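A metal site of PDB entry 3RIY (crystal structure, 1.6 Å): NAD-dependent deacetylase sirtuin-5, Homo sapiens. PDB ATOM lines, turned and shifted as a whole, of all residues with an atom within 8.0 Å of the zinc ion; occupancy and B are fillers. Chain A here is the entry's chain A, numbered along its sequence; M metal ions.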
ATOM      1  N   ARG A 136     -10.885  23.745  18.488  1.00  0.00           N
ATOM      2  CA  ARG A 136     -10.723  23.437  17.069  1.00  0.00           C
ATOM      3  C   ARG A 136     -10.612  24.746  16.302  1.00  0.00           C
ATOM      4  O   ARG A 136     -11.388  25.666  16.549  1.00  0.00           O
ATOM      5  CB  ARG A 136     -11.886  22.597  16.559  1.00  0.00           C
ATOM      6  CG  ARG A 136     -11.680  22.270  15.099  1.00  0.00           C
ATOM      7  CD  ARG A 136     -12.536  21.215  14.521  1.00  0.00           C
ATOM      8  NE  ARG A 136     -13.884  21.701  14.253  1.00  0.00           N
ATOM      9  CZ  ARG A 136     -14.943  21.352  14.967  1.00  0.00           C
ATOM     10  NH1 ARG A 136     -14.786  20.726  16.107  1.00  0.00           N
ATOM     11  NH2 ARG A 136     -16.175  21.714  14.594  1.00  0.00           N
ATOM     12  N   CYS A 137      -9.623  24.851  15.384  1.00  0.00           N
ATOM     13  CA  CYS A 137      -9.501  26.089  14.617  1.00  0.00           C
ATOM     14  C   CYS A 137     -10.520  26.134  13.481  1.00  0.00           C
ATOM     15  O   CYS A 137     -10.581  25.192  12.651  1.00  0.00           O
ATOM     16  CB  CYS A 137      -8.100  26.219  14.116  1.00  0.00           C
ATOM     17  SG  CYS A 137      -7.903  27.782  13.162  1.00  0.00           S
ATOM     18  N   THR A 138     -11.267  27.203  13.440  1.00  0.00           N
ATOM     19  CA  THR A 138     -12.270  27.408  12.359  1.00  0.00           C
ATOM     20  C   THR A 138     -11.620  27.731  11.004  1.00  0.00           C
ATOM     21  O   THR A 138     -12.339  27.700   9.985  1.00  0.00           O
ATOM     22  CB  THR A 138     -13.306  28.504  12.612  1.00  0.00           C
ATOM     23  OG1 THR A 138     -12.625  29.751  12.712  1.00  0.00           O
ATOM     24  CG2 THR A 138     -14.105  28.205  13.936  1.00  0.00           C
ATOM     25  N   SER A 139     -10.324  28.038  11.009  1.00  0.00           N
ATOM     26  CA  SER A 139      -9.529  28.248   9.748  1.00  0.00           C
ATOM     27  C   SER A 139      -8.773  27.013   9.253  1.00  0.00           C
ATOM     28  O   SER A 139      -9.074  26.571   8.154  1.00  0.00           O
ATOM     29  CB  SER A 139      -8.617  29.501   9.885  1.00  0.00           C
ATOM     30  OG  SER A 139      -7.910  29.756   8.675  1.00  0.00           O
ATOM     31  N   CYS A 140      -7.872  26.381  10.068  1.00  0.00           N
ATOM     32  CA  CYS A 140      -7.047  25.283   9.584  1.00  0.00           C
ATOM     33  C   CYS A 140      -7.585  23.925  10.061  1.00  0.00           C
ATOM     34  O   CYS A 140      -7.081  22.887   9.614  1.00  0.00           O
ATOM     35  CB  CYS A 140      -5.592  25.499   9.971  1.00  0.00           C
ATOM     36  SG  CYS A 140      -5.350  25.313  11.813  1.00  0.00           S
ATOM     37  N   GLY A 141      -8.584  23.905  10.964  1.00  0.00           N
ATOM     38  CA  GLY A 141      -9.175  22.634  11.436  1.00  0.00           C
ATOM     39  C   GLY A 141      -8.417  21.903  12.554  1.00  0.00           C
ATOM     40  O   GLY A 141      -8.861  20.848  13.009  1.00  0.00           O
ATOM     41  N   VAL A 142      -7.276  22.440  13.002  1.00  0.00           N
ATOM     42  CA  VAL A 142      -6.468  21.687  13.941  1.00  0.00           C
ATOM     43  C   VAL A 142      -7.173  21.639  15.332  1.00  0.00           C
ATOM     44  O   VAL A 142      -7.742  22.614  15.767  1.00  0.00           O
ATOM     45  CB  VAL A 142      -5.046  22.303  14.088  1.00  0.00           C
ATOM     46  CG1 VAL A 142      -5.043  23.607  14.745  1.00  0.00           C
ATOM     47  CG2 VAL A 142      -4.212  21.458  14.980  1.00  0.00           C
ATOM     48  N   VAL A 143      -7.098  20.490  15.968  1.00  0.00           N
ATOM     49  CA  VAL A 143      -7.697  20.258  17.274  1.00  0.00           C
ATOM     50  C   VAL A 143      -6.519  20.209  18.259  1.00  0.00           C
ATOM     51  O   VAL A 143      -5.484  19.534  18.014  1.00  0.00           O
ATOM     52  CB  VAL A 143      -8.425  18.887  17.242  1.00  0.00           C
ATOM     53  CG1 VAL A 143      -8.899  18.498  18.627  1.00  0.00           C
ATOM     54  CG2 VAL A 143      -9.614  19.006  16.258  1.00  0.00           C
ATOM     55  N   ARG A 177      -7.382  32.542  19.677  1.00  0.00           N
ATOM     56  CA  ARG A 177      -6.851  32.444  18.297  1.00  0.00           C
ATOM     57  C   ARG A 177      -5.862  31.290  18.141  1.00  0.00           C
ATOM     58  O   ARG A 177      -5.119  30.943  19.075  1.00  0.00           O
ATOM     59  CB  ARG A 177      -6.139  33.764  17.840  1.00  0.00           C
ATOM     60  CG  ARG A 177      -6.981  35.025  18.052  1.00  0.00           C
ATOM     61  CD  ARG A 177      -8.339  35.020  17.344  1.00  0.00           C
ATOM     62  NE  ARG A 177      -8.224  34.945  15.872  1.00  0.00           N
ATOM     63  CZ  ARG A 177      -9.144  35.413  15.024  1.00  0.00           C
ATOM     64  NH1 ARG A 177     -10.264  36.021  15.449  1.00  0.00           N
ATOM     65  NH2 ARG A 177      -8.932  35.282  13.738  1.00  0.00           N
ATOM     66  N   CYS A 178      -5.812  30.777  16.927  1.00  0.00           N
ATOM     67  CA  CYS A 178      -4.920  29.631  16.586  1.00  0.00           C
ATOM     68  C   CYS A 178      -3.442  30.001  16.587  1.00  0.00           C
ATOM     69  O   CYS A 178      -3.073  30.949  15.945  1.00  0.00           O
ATOM     70  CB  CYS A 178      -5.309  29.108  15.192  1.00  0.00           C
ATOM     71  SG  CYS A 178      -4.430  27.584  14.764  1.00  0.00           S
ATOM     72  N   GLU A 179      -2.600  29.249  17.262  1.00  0.00           N
ATOM     73  CA  GLU A 179      -1.184  29.521  17.324  1.00  0.00           C
ATOM     74  C   GLU A 179      -0.384  28.551  16.489  1.00  0.00           C
ATOM     75  O   GLU A 179       0.838  28.572  16.587  1.00  0.00           O
ATOM     76  CB  GLU A 179      -0.696  29.426  18.778  1.00  0.00           C
ATOM     77  CG  GLU A 179      -1.354  30.500  19.558  1.00  0.00           C
ATOM     78  CD  GLU A 179      -0.963  30.632  21.013  1.00  0.00           C
ATOM     79  OE1 GLU A 179      -0.243  29.759  21.573  1.00  0.00           O
ATOM     80  OE2 GLU A 179      -1.440  31.636  21.607  1.00  0.00           O
ATOM     81  N   GLU A 180      -1.037  27.734  15.677  1.00  0.00           N
ATOM     82  CA  GLU A 180      -0.358  26.600  15.010  1.00  0.00           C
ATOM     83  C   GLU A 180       0.226  27.139  13.710  1.00  0.00           C
ATOM     84  O   GLU A 180      -0.553  27.657  12.917  1.00  0.00           O
ATOM     85  CB  GLU A 180      -1.385  25.469  14.675  1.00  0.00           C
ATOM     86  CG  GLU A 180      -0.782  24.374  13.832  1.00  0.00           C
ATOM     87  CD  GLU A 180      -0.079  23.377  14.699  1.00  0.00           C
ATOM     88  OE1 GLU A 180       1.146  23.184  14.534  1.00  0.00           O
ATOM     89  OE2 GLU A 180      -0.775  22.821  15.582  1.00  0.00           O
ATOM     90  N   ALA A 181       1.557  26.990  13.483  1.00  0.00           N
ATOM     91  CA  ALA A 181       2.241  27.449  12.224  1.00  0.00           C
ATOM     92  C   ALA A 181       1.817  28.881  11.875  1.00  0.00           C
ATOM     93  O   ALA A 181       1.630  29.255  10.731  1.00  0.00           O
ATOM     94  CB  ALA A 181       2.015  26.468  11.046  1.00  0.00           C
ATOM     95  N   GLY A 182       1.704  29.686  12.910  1.00  0.00           N
ATOM     96  CA  GLY A 182       1.317  31.097  12.766  1.00  0.00           C
ATOM     97  C   GLY A 182      -0.045  31.326  12.119  1.00  0.00           C
ATOM     98  O   GLY A 182      -0.282  32.409  11.581  1.00  0.00           O
ATOM     99  N   CYS A 183      -0.970  30.347  12.185  1.00  0.00           N
ATOM    100  CA  CYS A 183      -2.293  30.456  11.474  1.00  0.00           C
ATOM    101  C   CYS A 183      -3.127  31.711  11.862  1.00  0.00           C
ATOM    102  O   CYS A 183      -3.670  32.380  10.978  1.00  0.00           O
ATOM    103  CB  CYS A 183      -3.133  29.192  11.729  1.00  0.00           C
ATOM    104  SG  CYS A 183      -4.989  29.271  11.357  1.00  0.00           S
ATOM    105  N   GLY A 184      -3.280  31.968  13.177  1.00  0.00           N
ATOM    106  CA  GLY A 184      -4.122  33.051  13.669  1.00  0.00           C
ATOM    107  C   GLY A 184      -5.651  32.966  13.571  1.00  0.00           C
ATOM    108  O   GLY A 184      -6.339  33.931  13.974  1.00  0.00           O
ATOM    109  N   GLY A 185      -6.204  31.849  13.050  1.00  0.00           N
ATOM    110  CA  GLY A 185      -7.678  31.737  12.916  1.00  0.00           C
ATOM    111  C   GLY A 185      -8.468  31.723  14.219  1.00  0.00           C
ATOM    112  O   GLY A 185      -7.909  31.482  15.267  1.00  0.00           O
ATOM    113  N   LEU A 186      -9.744  32.027  14.155  1.00  0.00           N
ATOM    114  CA  LEU A 186     -10.615  31.990  15.344  1.00  0.00           C
ATOM    115  C   LEU A 186     -10.799  30.551  15.824  1.00  0.00           C
ATOM    116  O   LEU A 186     -11.251  29.687  15.044  1.00  0.00           O
ATOM    117  CB  LEU A 186     -11.989  32.598  15.013  1.00  0.00           C
ATOM    118  CG  LEU A 186     -13.004  32.551  16.142  1.00  0.00           C
ATOM    119  CD1 LEU A 186     -12.513  33.350  17.410  1.00  0.00           C
ATOM    120  CD2 LEU A 186     -14.418  33.062  15.632  1.00  0.00           C
ATOM    121  N   LEU A 187     -10.535  30.275  17.094  1.00  0.00           N
ATOM    122  CA  LEU A 187     -10.816  28.964  17.665  1.00  0.00           C
ATOM    123  C   LEU A 187     -12.199  28.866  18.143  1.00  0.00           C
ATOM    124  O   LEU A 187     -12.819  29.874  18.537  1.00  0.00           O
ATOM    125  CB  LEU A 187      -9.915  28.703  18.880  1.00  0.00           C
ATOM    126  CG  LEU A 187      -8.420  28.786  18.626  1.00  0.00           C
ATOM    127  CD1 LEU A 187      -7.632  28.374  19.857  1.00  0.00           C
ATOM    128  CD2 LEU A 187      -8.010  27.813  17.424  1.00  0.00           C
HETATM  129 ZN    ZN M   1      -5.612  27.439  12.708  1.00  0.00          ZN
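The side-chain sulfur (SG) of Cys 140 sits close to the backbone NH (N) of Val 142 (3.7 Å). SG of Cys 183 sits close to N of Gly 185. The backbone NH (N) of Cys 137 lies within hydrogen-bond range of the backbone carbonyl oxygen (O) of Val 142. SG of Cys 137 sits close to N of Ser 139 (3.2 Å). The backbone carbonyl oxygen (O) of Gly 185 sits at hydrogen-bond distance from the backbone NH (N) of Cys 178 (2.8 Å). The side-chain sulfur (SG) of Cys 178 sits close to the backbone NH (N) of Glu 180 (3.5 Å). O of Cys 178 is in hydrogen-bond range of N of Gly 184 (3.0 Å).
Four residues have an atom within 4 Å of the zinc ion: Cys 137, Cys 140, Cys 178 and Cys 183.
The zinc ion is bound by the side-chain sulfur of Cys 140 (2.3 Å), the side-chain sulfur of Cys 183 (2.4 Å), the side-chain sulfur of Cys 137 (2.4 Å) and the side-chain sulfur of Cys 178 (2.4 Å). The zinc ion has four donor atoms within binding distance.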
